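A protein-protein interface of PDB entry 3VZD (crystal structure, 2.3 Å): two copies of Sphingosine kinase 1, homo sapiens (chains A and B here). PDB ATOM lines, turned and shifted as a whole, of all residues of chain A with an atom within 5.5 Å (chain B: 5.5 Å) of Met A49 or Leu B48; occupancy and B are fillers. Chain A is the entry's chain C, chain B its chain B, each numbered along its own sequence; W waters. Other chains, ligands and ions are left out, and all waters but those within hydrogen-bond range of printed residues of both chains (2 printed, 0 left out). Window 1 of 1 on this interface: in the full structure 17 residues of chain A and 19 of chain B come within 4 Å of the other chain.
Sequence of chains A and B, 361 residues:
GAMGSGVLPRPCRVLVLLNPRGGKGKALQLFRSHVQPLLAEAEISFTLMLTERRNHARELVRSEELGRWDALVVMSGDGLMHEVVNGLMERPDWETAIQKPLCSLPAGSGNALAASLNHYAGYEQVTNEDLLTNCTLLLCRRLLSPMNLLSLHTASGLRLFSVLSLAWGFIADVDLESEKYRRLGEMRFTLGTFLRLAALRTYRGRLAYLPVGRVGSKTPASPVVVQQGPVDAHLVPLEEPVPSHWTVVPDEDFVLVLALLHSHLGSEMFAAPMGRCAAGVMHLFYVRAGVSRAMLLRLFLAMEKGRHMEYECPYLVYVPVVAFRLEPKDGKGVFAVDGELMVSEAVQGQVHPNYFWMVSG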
ATOM      1  N   LEU A  15      23.671 -23.239  18.012  1.00  0.00           N
ATOM      2  CA  LEU A  15      23.338 -22.357  19.098  1.00  0.00           C
ATOM      3  C   LEU A  15      24.185 -22.679  20.323  1.00  0.00           C
ATOM      4  O   LEU A  15      24.215 -23.844  20.740  1.00  0.00           O
ATOM      5  CB  LEU A  15      21.874 -22.497  19.465  1.00  0.00           C
ATOM      6  CG  LEU A  15      21.330 -21.696  20.672  1.00  0.00           C
ATOM      7  CD1 LEU A  15      21.530 -20.198  20.501  1.00  0.00           C
ATOM      8  CD2 LEU A  15      19.841 -22.006  20.876  1.00  0.00           C
ATOM      9  N   VAL A  16      24.861 -21.682  20.905  1.00  0.00           N
ATOM     10  CA  VAL A  16      25.664 -21.925  22.049  1.00  0.00           C
ATOM     11  C   VAL A  16      25.016 -21.203  23.227  1.00  0.00           C
ATOM     12  O   VAL A  16      24.886 -19.972  23.203  1.00  0.00           O
ATOM     13  CB  VAL A  16      27.144 -21.463  21.843  1.00  0.00           C
ATOM     14  CG1 VAL A  16      27.980 -21.711  23.103  1.00  0.00           C
ATOM     15  CG2 VAL A  16      27.809 -22.237  20.705  1.00  0.00           C
ATOM     16  N   LEU A  17      24.605 -21.953  24.241  1.00  0.00           N
ATOM     17  CA  LEU A  17      24.014 -21.401  25.410  1.00  0.00           C
ATOM     18  C   LEU A  17      25.058 -21.392  26.487  1.00  0.00           C
ATOM     19  O   LEU A  17      25.583 -22.449  26.871  1.00  0.00           O
ATOM     20  CB  LEU A  17      22.816 -22.225  25.862  1.00  0.00           C
ATOM     21  CG  LEU A  17      21.680 -22.264  24.824  1.00  0.00           C
ATOM     22  CD1 LEU A  17      20.776 -23.351  25.120  1.00  0.00           C
ATOM     23  CD2 LEU A  17      20.872 -20.956  24.885  1.00  0.00           C
ATOM     24  N   LEU A  18      25.378 -20.214  26.984  1.00  0.00           N
ATOM     25  CA  LEU A  18      26.525 -20.123  27.843  1.00  0.00           C
ATOM     26  C   LEU A  18      26.106 -19.471  29.130  1.00  0.00           C
ATOM     27  O   LEU A  18      25.333 -18.513  29.108  1.00  0.00           O
ATOM     28  CB  LEU A  18      27.625 -19.352  27.127  1.00  0.00           C
ATOM     29  CG  LEU A  18      28.938 -19.185  27.853  1.00  0.00           C
ATOM     30  CD1 LEU A  18      30.022 -19.144  26.799  1.00  0.00           C
ATOM     31  CD2 LEU A  18      29.002 -17.907  28.698  1.00  0.00           C
ATOM     32  N   THR A  47      25.948 -18.939  17.236  1.00  0.00           N
ATOM     33  CA  THR A  47      25.550 -17.771  17.954  1.00  0.00           C
ATOM     34  C   THR A  47      25.510 -18.042  19.426  1.00  0.00           C
ATOM     35  O   THR A  47      25.002 -19.091  19.857  1.00  0.00           O
ATOM     36  CB  THR A  47      24.280 -17.036  17.357  1.00  0.00           C
ATOM     37  OG1 THR A  47      23.218 -16.934  18.300  1.00  0.00           O
ATOM     38  CG2 THR A  47      23.814 -17.614  16.179  1.00  0.00           C
ATOM     39  N   LEU A  48      26.121 -17.137  20.193  1.00  0.00           N
ATOM     40  CA  LEU A  48      26.071 -17.196  21.653  1.00  0.00           C
ATOM     41  C   LEU A  48      24.770 -16.552  22.179  1.00  0.00           C
ATOM     42  O   LEU A  48      24.407 -15.435  21.754  1.00  0.00           O
ATOM     43  CB  LEU A  48      27.230 -16.437  22.263  1.00  0.00           C
ATOM     44  CG  LEU A  48      28.614 -17.075  22.411  1.00  0.00           C
ATOM     45  CD1 LEU A  48      29.667 -15.980  22.702  1.00  0.00           C
ATOM     46  CD2 LEU A  48      28.605 -18.111  23.513  1.00  0.00           C
ATOM     47  N   MET A  49      24.077 -17.252  23.064  1.00  0.00           N
ATOM     48  CA  MET A  49      23.098 -16.650  23.939  1.00  0.00           C
ATOM     49  C   MET A  49      23.574 -16.952  25.329  1.00  0.00           C
ATOM     50  O   MET A  49      24.063 -18.054  25.619  1.00  0.00           O
ATOM     51  CB  MET A  49      21.678 -17.199  23.767  1.00  0.00           C
ATOM     52  CG  MET A  49      21.025 -16.992  22.384  1.00  0.00           C
ATOM     53  SD  MET A  49      19.192 -17.274  22.408  1.00  0.00           S
ATOM     54  CE  MET A  49      18.976 -18.243  20.960  1.00  0.00           C
ATOM     55  N   LEU A  50      23.402 -15.974  26.205  1.00  0.00           N
ATOM     56  CA  LEU A  50      23.828 -16.055  27.585  1.00  0.00           C
ATOM     57  C   LEU A  50      22.648 -16.388  28.441  1.00  0.00           C
ATOM     58  O   LEU A  50      21.563 -15.859  28.233  1.00  0.00           O
ATOM     59  CB  LEU A  50      24.456 -14.744  28.044  1.00  0.00           C
ATOM     60  CG  LEU A  50      25.661 -14.200  27.238  1.00  0.00           C
ATOM     61  CD1 LEU A  50      26.425 -13.103  28.014  1.00  0.00           C
ATOM     62  CD2 LEU A  50      26.633 -15.267  26.757  1.00  0.00           C
ATOM     63  N   THR A  51      22.829 -17.297  29.397  1.00  0.00           N
ATOM     64  CA  THR A  51      21.734 -17.595  30.286  1.00  0.00           C
ATOM     65  C   THR A  51      21.888 -16.726  31.510  1.00  0.00           C
ATOM     66  O   THR A  51      23.003 -16.368  31.881  1.00  0.00           O
ATOM     67  CB  THR A  51      21.709 -19.076  30.738  1.00  0.00           C
ATOM     68  OG1 THR A  51      22.886 -19.382  31.542  1.00  0.00           O
ATOM     69  CG2 THR A  51      21.581 -19.989  29.526  1.00  0.00           C
ATOM     70  N   GLU A  52      20.771 -16.418  32.160  1.00  0.00           N
ATOM     71  CA  GLU A  52      20.737 -15.341  33.158  1.00  0.00           C
ATOM     72  C   GLU A  52      20.237 -15.795  34.539  1.00  0.00           C
ATOM     73  O   GLU A  52      20.404 -15.064  35.523  1.00  0.00           O
ATOM     74  CB  GLU A  52      19.862 -14.173  32.634  1.00  0.00           C
ATOM     75  CG  GLU A  52      20.497 -13.419  31.473  1.00  0.00           C
ATOM     76  CD  GLU A  52      21.894 -12.858  31.800  1.00  0.00           C
ATOM     77  OE1 GLU A  52      22.788 -12.908  30.938  1.00  0.00           O
ATOM     78  OE2 GLU A  52      22.104 -12.405  32.945  1.00  0.00           O
ATOM     79  N   HIS A  56      16.154 -20.464  32.589  1.00  0.00           N
ATOM     80  CA  HIS A  56      16.246 -19.660  31.432  1.00  0.00           C
ATOM     81  C   HIS A  56      16.580 -20.512  30.185  1.00  0.00           C
ATOM     82  O   HIS A  56      15.940 -20.388  29.177  1.00  0.00           O
ATOM     83  CB  HIS A  56      17.298 -18.571  31.651  1.00  0.00           C
ATOM     84  CG  HIS A  56      17.324 -17.545  30.566  1.00  0.00           C
ATOM     85  ND1 HIS A  56      18.348 -16.628  30.426  1.00  0.00           N
ATOM     86  CD2 HIS A  56      16.435 -17.270  29.579  1.00  0.00           C
ATOM     87  CE1 HIS A  56      18.096 -15.844  29.391  1.00  0.00           C
ATOM     88  NE2 HIS A  56      16.932 -16.200  28.874  1.00  0.00           N
ATOM     89  N   LEU A  60      14.168 -21.049  26.814  1.00  0.00           N
ATOM     90  CA  LEU A  60      14.645 -20.722  25.455  1.00  0.00           C
ATOM     91  C   LEU A  60      14.490 -21.926  24.497  1.00  0.00           C
ATOM     92  O   LEU A  60      14.077 -21.793  23.349  1.00  0.00           O
ATOM     93  CB  LEU A  60      16.091 -20.254  25.504  1.00  0.00           C
ATOM     94  CG  LEU A  60      16.357 -18.783  25.920  1.00  0.00           C
ATOM     95  CD1 LEU A  60      17.826 -18.590  26.362  1.00  0.00           C
ATOM     96  CD2 LEU A  60      15.976 -17.775  24.818  1.00  0.00           C
ATOM     97  N   GLU A  64      12.280 -22.324  21.235  1.00  0.00           N
ATOM     98  CA  GLU A  64      13.211 -22.147  20.107  1.00  0.00           C
ATOM     99  C   GLU A  64      12.656 -22.703  18.792  1.00  0.00           C
ATOM    100  O   GLU A  64      11.882 -23.694  18.766  1.00  0.00           O
ATOM    101  CB  GLU A  64      14.577 -22.759  20.419  1.00  0.00           C
ATOM    102  CG  GLU A  64      15.711 -22.368  19.484  1.00  0.00           C
ATOM    103  CD  GLU A  64      16.267 -20.902  19.625  1.00  0.00           C
ATOM    104  OE1 GLU A  64      16.495 -20.325  20.746  1.00  0.00           O
ATOM    105  OE2 GLU A  64      16.600 -20.358  18.580  1.00  0.00           O
ATOM    106  N   ARG A  68      16.694 -23.850  12.636  1.00  0.00           N
ATOM    107  CA  ARG A  68      17.820 -22.925  12.433  1.00  0.00           C
ATOM    108  C   ARG A  68      19.158 -23.529  12.838  1.00  0.00           C
ATOM    109  O   ARG A  68      20.197 -22.979  12.533  1.00  0.00           O
ATOM    110  CB  ARG A  68      17.707 -21.798  13.484  1.00  0.00           C
ATOM    111  CG  ARG A  68      16.921 -20.524  13.192  1.00  0.00           C
ATOM    112  CD  ARG A  68      16.580 -19.935  14.591  1.00  0.00           C
ATOM    113  NE  ARG A  68      16.630 -18.477  14.589  1.00  0.00           N
ATOM    114  CZ  ARG A  68      16.713 -17.743  15.689  1.00  0.00           C
ATOM    115  NH1 ARG A  68      16.804 -18.315  16.861  1.00  0.00           N
ATOM    116  NH2 ARG A  68      16.762 -16.430  15.601  1.00  0.00           N
ATOM    117  N   TRP A  69      19.153 -24.547  13.685  1.00  0.00           N
ATOM    118  CA  TRP A  69      20.406 -24.970  14.337  1.00  0.00           C
ATOM    119  C   TRP A  69      20.702 -26.406  13.903  1.00  0.00           C
ATOM    120  O   TRP A  69      19.770 -27.211  13.742  1.00  0.00           O
ATOM    121  CB  TRP A  69      20.274 -24.884  15.878  1.00  0.00           C
ATOM    122  CG  TRP A  69      19.871 -23.504  16.322  1.00  0.00           C
ATOM    123  CD1 TRP A  69      18.733 -23.144  16.985  1.00  0.00           C
ATOM    124  CD2 TRP A  69      20.586 -22.303  16.068  1.00  0.00           C
ATOM    125  NE1 TRP A  69      18.718 -21.799  17.191  1.00  0.00           N
ATOM    126  CE2 TRP A  69      19.843 -21.254  16.626  1.00  0.00           C
ATOM    127  CE3 TRP A  69      21.801 -22.013  15.419  1.00  0.00           C
ATOM    128  CZ2 TRP A  69      20.257 -19.910  16.556  1.00  0.00           C
ATOM    129  CZ3 TRP A  69      22.228 -20.677  15.356  1.00  0.00           C
ATOM    130  CH2 TRP A  69      21.453 -19.652  15.918  1.00  0.00           C
ATOM    131  N   LEU B  15      14.473  -9.662  23.899  1.00  0.00           N
ATOM    132  CA  LEU B  15      15.698 -10.107  23.273  1.00  0.00           C
ATOM    133  C   LEU B  15      16.625  -8.921  23.111  1.00  0.00           C
ATOM    134  O   LEU B  15      16.274  -7.956  22.440  1.00  0.00           O
ATOM    135  CB  LEU B  15      15.400 -10.738  21.894  1.00  0.00           C
ATOM    136  CG  LEU B  15      16.556 -11.285  21.061  1.00  0.00           C
ATOM    137  CD1 LEU B  15      17.284 -12.398  21.852  1.00  0.00           C
ATOM    138  CD2 LEU B  15      16.089 -11.782  19.672  1.00  0.00           C
ATOM    139  N   VAL B  16      17.814  -9.016  23.692  1.00  0.00           N
ATOM    140  CA  VAL B  16      18.819  -8.004  23.528  1.00  0.00           C
ATOM    141  C   VAL B  16      19.925  -8.501  22.555  1.00  0.00           C
ATOM    142  O   VAL B  16      20.735  -9.368  22.898  1.00  0.00           O
ATOM    143  CB  VAL B  16      19.416  -7.565  24.912  1.00  0.00           C
ATOM    144  CG1 VAL B  16      20.463  -6.452  24.706  1.00  0.00           C
ATOM    145  CG2 VAL B  16      18.301  -7.043  25.873  1.00  0.00           C
ATOM    146  N   LEU B  18      23.117  -7.634  21.087  1.00  0.00           N
ATOM    147  CA  LEU B  18      24.225  -6.789  21.463  1.00  0.00           C
ATOM    148  C   LEU B  18      25.497  -7.134  20.682  1.00  0.00           C
ATOM    149  O   LEU B  18      25.866  -8.339  20.534  1.00  0.00           O
ATOM    150  CB  LEU B  18      24.500  -6.955  22.975  1.00  0.00           C
ATOM    151  CG  LEU B  18      25.608  -6.141  23.653  1.00  0.00           C
ATOM    152  CD1 LEU B  18      25.245  -5.944  25.137  1.00  0.00           C
ATOM    153  CD2 LEU B  18      26.979  -6.852  23.595  1.00  0.00           C
ATOM    154  N   LEU B  28      29.117  -5.012  26.172  1.00  0.00           N
ATOM    155  CA  LEU B  28      28.608  -5.971  27.122  1.00  0.00           C
ATOM    156  C   LEU B  28      28.777  -5.531  28.603  1.00  0.00           C
ATOM    157  O   LEU B  28      27.826  -5.660  29.424  1.00  0.00           O
ATOM    158  CB  LEU B  28      29.187  -7.379  26.824  1.00  0.00           C
ATOM    159  CG  LEU B  28      28.726  -8.497  27.771  1.00  0.00           C
ATOM    160  CD1 LEU B  28      27.192  -8.730  27.698  1.00  0.00           C
ATOM    161  CD2 LEU B  28      29.419  -9.799  27.428  1.00  0.00           C
ATOM    162  N   PHE B  31      26.255  -2.806  29.324  1.00  0.00           N
ATOM    163  CA  PHE B  31      24.950  -3.435  29.518  1.00  0.00           C
ATOM    164  C   PHE B  31      24.825  -3.884  30.961  1.00  0.00           C
ATOM    165  O   PHE B  31      23.829  -3.736  31.609  1.00  0.00           O
ATOM    166  CB  PHE B  31      24.726  -4.632  28.592  1.00  0.00           C
ATOM    167  CG  PHE B  31      23.445  -5.359  28.895  1.00  0.00           C
ATOM    168  CD1 PHE B  31      22.241  -4.907  28.370  1.00  0.00           C
ATOM    169  CD2 PHE B  31      23.422  -6.422  29.773  1.00  0.00           C
ATOM    170  CE1 PHE B  31      21.064  -5.526  28.690  1.00  0.00           C
ATOM    171  CE2 PHE B  31      22.190  -7.041  30.136  1.00  0.00           C
ATOM    172  CZ  PHE B  31      21.052  -6.623  29.562  1.00  0.00           C
ATOM    173  N   ARG B  32      25.866  -4.521  31.416  1.00  0.00           N
ATOM    174  CA  ARG B  32      25.890  -5.120  32.712  1.00  0.00           C
ATOM    175  C   ARG B  32      25.850  -4.031  33.786  1.00  0.00           C
ATOM    176  O   ARG B  32      25.125  -4.140  34.772  1.00  0.00           O
ATOM    177  CB  ARG B  32      27.220  -5.901  32.797  1.00  0.00           C
ATOM    178  CG  ARG B  32      27.174  -7.324  33.169  1.00  0.00           C
ATOM    179  CD  ARG B  32      26.889  -8.353  32.054  1.00  0.00           C
ATOM    180  NE  ARG B  32      25.603  -8.945  32.413  1.00  0.00           N
ATOM    181  CZ  ARG B  32      25.049 -10.071  31.953  1.00  0.00           C
ATOM    182  NH1 ARG B  32      25.635 -10.871  31.098  1.00  0.00           N
ATOM    183  NH2 ARG B  32      23.859 -10.371  32.388  1.00  0.00           N
ATOM    184  N   PHE B  46      15.429 -10.512  30.126  1.00  0.00           N
ATOM    185  CA  PHE B  46      16.043 -10.343  28.833  1.00  0.00           C
ATOM    186  C   PHE B  46      16.879 -11.612  28.533  1.00  0.00           C
ATOM    187  O   PHE B  46      17.304 -12.358  29.448  1.00  0.00           O
ATOM    188  CB  PHE B  46      16.987  -9.099  28.886  1.00  0.00           C
ATOM    189  CG  PHE B  46      18.041  -9.234  29.901  1.00  0.00           C
ATOM    190  CD1 PHE B  46      17.816  -8.835  31.207  1.00  0.00           C
ATOM    191  CD2 PHE B  46      19.250  -9.811  29.569  1.00  0.00           C
ATOM    192  CE1 PHE B  46      18.787  -9.011  32.189  1.00  0.00           C
ATOM    193  CE2 PHE B  46      20.231  -9.963  30.508  1.00  0.00           C
ATOM    194  CZ  PHE B  46      19.991  -9.571  31.857  1.00  0.00           C
ATOM    195  N   THR B  47      17.120 -11.837  27.253  1.00  0.00           N
ATOM    196  CA  THR B  47      18.157 -12.717  26.850  1.00  0.00           C
ATOM    197  C   THR B  47      19.073 -12.020  25.870  1.00  0.00           C
ATOM    198  O   THR B  47      18.629 -11.289  24.998  1.00  0.00           O
ATOM    199  CB  THR B  47      17.718 -14.229  26.566  1.00  0.00           C
ATOM    200  OG1 THR B  47      18.260 -14.725  25.341  1.00  0.00           O
ATOM    201  CG2 THR B  47      16.330 -14.431  26.568  1.00  0.00           C
ATOM    202  N   LEU B  48      20.353 -12.103  26.184  1.00  0.00           N
ATOM    203  CA  LEU B  48      21.413 -11.602  25.375  1.00  0.00           C
ATOM    204  C   LEU B  48      21.855 -12.573  24.320  1.00  0.00           C
ATOM    205  O   LEU B  48      22.179 -13.719  24.591  1.00  0.00           O
ATOM    206  CB  LEU B  48      22.661 -11.255  26.210  1.00  0.00           C
ATOM    207  CG  LEU B  48      22.566 -10.088  27.184  1.00  0.00           C
ATOM    208  CD1 LEU B  48      23.610 -10.272  28.299  1.00  0.00           C
ATOM    209  CD2 LEU B  48      22.759  -8.736  26.475  1.00  0.00           C
ATOM    210  N   MET B  49      21.899 -12.060  23.122  1.00  0.00           N
ATOM    211  CA  MET B  49      22.441 -12.718  21.995  1.00  0.00           C
ATOM    212  C   MET B  49      23.545 -11.805  21.383  1.00  0.00           C
ATOM    213  O   MET B  49      23.300 -10.623  21.047  1.00  0.00           O
ATOM    214  CB  MET B  49      21.287 -12.943  21.069  1.00  0.00           C
ATOM    215  CG  MET B  49      21.569 -13.700  19.850  1.00  0.00           C
ATOM    216  SD  MET B  49      19.995 -14.036  18.911  1.00  0.00           S
ATOM    217  CE  MET B  49      19.164 -15.245  19.998  1.00  0.00           C
ATOM    218  N   LEU B  50      24.758 -12.330  21.277  1.00  0.00           N
ATOM    219  CA  LEU B  50      25.883 -11.551  20.811  1.00  0.00           C
ATOM    220  C   LEU B  50      25.977 -11.635  19.303  1.00  0.00           C
ATOM    221  O   LEU B  50      25.835 -12.722  18.729  1.00  0.00           O
ATOM    222  CB  LEU B  50      27.178 -11.992  21.482  1.00  0.00           C
ATOM    223  CG  LEU B  50      27.146 -12.077  23.001  1.00  0.00           C
ATOM    224  CD1 LEU B  50      28.479 -12.534  23.569  1.00  0.00           C
ATOM    225  CD2 LEU B  50      26.812 -10.812  23.701  1.00  0.00           C
ATOM    226  N   ARG B  68       7.973 -15.317  21.164  1.00  0.00           N
ATOM    227  CA  ARG B  68       8.553 -15.432  22.496  1.00  0.00           C
ATOM    228  C   ARG B  68       8.945 -14.054  23.039  1.00  0.00           C
ATOM    229  O   ARG B  68       9.240 -13.938  24.215  1.00  0.00           O
ATOM    230  CB  ARG B  68       9.824 -16.318  22.497  1.00  0.00           C
ATOM    231  CG  ARG B  68      10.289 -16.695  21.136  1.00  0.00           C
ATOM    232  CD  ARG B  68      11.803 -16.722  20.906  1.00  0.00           C
ATOM    233  NE  ARG B  68      12.265 -17.894  21.516  1.00  0.00           N
ATOM    234  CZ  ARG B  68      13.500 -18.349  21.473  1.00  0.00           C
ATOM    235  NH1 ARG B  68      14.456 -17.707  20.839  1.00  0.00           N
ATOM    236  NH2 ARG B  68      13.755 -19.466  22.117  1.00  0.00           N
HETATM  237  O   HOH W   1      27.409 -14.894  18.898  1.00  0.00           O
HETATM  238  O   HOH W   2      21.019 -13.127  28.487  1.00  0.00           O
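OE2 of Glu A52 lies within salt-bridge range of NH2 of Arg B32 (2.7 Å).
The backbone NH of Leu B50 is in hydrogen-bond range of the backbone carbonyl oxygen of Leu A48 (3.2 Å).
The backbone carbonyl oxygen of Leu B48 lies within hydrogen-bond range of the backbone NH of Leu A50 (3.0 Å).
The side-chain carboxylate (OE1) of Glu A64 lies within salt-bridge range of the guanidinium group (NH2) of Arg B68 (3.2 Å).
The guanidinium group of Arg B68 sits at hydrogen-bond distance from the backbone carbonyl oxygen of Leu A60 (2.7 Å).
N of Met B49 is in hydrogen-bond range of O of Val B16, 2.9 Å away.
The backbone carbonyl oxygen (O) of Met A49 lies within hydrogen-bond range of the backbone NH (N) of Leu A18, 2.9 Å away.
The backbone NH (N) of Leu B18 is in hydrogen-bond range of the backbone carbonyl oxygen (O) of Met B49, 3.0 Å away.
OE2 of Glu A64 sits at hydrogen-bond distance from NE1 of Trp A69, at 2.9 Å.
The guanidinium group of Arg A68 is in salt-bridge range of the side-chain carboxylate of Glu A64, at 2.7 Å.
O of Val A16 lies within hydrogen-bond range of N of Met A49 (2.8 Å).
OG1 of Thr A47 touches CG of Met B49, 3.9 Å away.
Leu A48 touches Leu B48.
CA of Met B49 touches O of Leu A48 (3.4 Å).
Met A49 touches Thr B47.
Leu B48 touches Met A49.
CE of Met B49 touches SD of Met A49, 3.2 Å away.
Leu A50 touches Arg B32.
CE2 of Phe B46 touches CD of Glu A52, 3.6 Å away.
Leu B48 touches Glu A52.
CE1 of His A56 touches O of Phe B46, at 3.6 Å.
Of the printed residues of chain B, Met A49 touches Thr B47 (3.996 Å), Leu B48 (3.1 Å) and Met B49 (3.2 Å).
Printed residues of chain A within 4 Å of Leu B48: Leu A48 (3.99 Å), Met A49 (3.1 Å), Leu A50 (3.0 Å) and Glu A52 (3.8 Å).
Of the printed residues of chain B, Thr A47 touches Met B49 (3.9 Å).
Of the printed residues of chain B, His A56 touches Phe B46 and Thr B47.
Printed residues of chain B within 4 Å of Leu A50: Arg B32 (3.9 Å) and Leu B48 (3.0 Å).
Of the printed residues of chain A, Arg B32 touches Leu A50 (3.9 Å) and Glu A52 (2.7 Å).
Phe B31 touches none of the printed residues of chain A.
Arg A68 touches none of the printed residues of chain B.
The nearest printed residue of chain B that does not touch Met A49 is Arg B68 (4.6 Å).
The nearest printed residue of chain A that does not touch Met B49 is Arg A68 (5.0 Å).
Of the 15 printed residues of chain A, 8 touch a printed residue of chain B.
Hydrophobic or aromatic side chains of chain A within 4 Å of the printed part of chain B: Leu A48, Met A49, Leu A50, His A56 and Leu A60.
Printed residues of chain B that touch a printed residue of chain A: Arg B32, Phe B46, Thr B47, Leu B48, Met B49, Leu B50 and Arg B68.
Hydrophobic or aromatic side chains of chain B within 4 Å of the printed part of chain A: Phe B46, Leu B48, Met B49 and Leu B50.
Among the printed residues, 17 pairs touch across the chains.
Thr A47 touches Met B49, and with the chains exchanged Met A49 touches Thr B47.
Leu A48 touches its own counterpart, Leu B48.
Leu A48 touches Met B49, and with the chains exchanged Met A49 touches Leu B48.
Met B49 touches its own counterpart, Met A49.
Positions printed for both chains: 15, 16, 18, 47, 48, 49, 50 and 68.
Of the 17 pairs that touch across the chains among the printed residues, 8 have their exchanged pair printed and touching as well.
Water W2 lies within hydrogen-bond range of the backbone NH (N) of Leu B48 (2.6 Å), the backbone carbonyl oxygen (O) of Leu A50 (2.8 Å) and the side-chain carboxylate (OE1) of Glu A52 (3.0 Å).
Water W1 lies within hydrogen-bond range of the backbone carbonyl oxygen of Leu B50 (2.7 Å) and the backbone NH of Leu A48 (2.9 Å).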
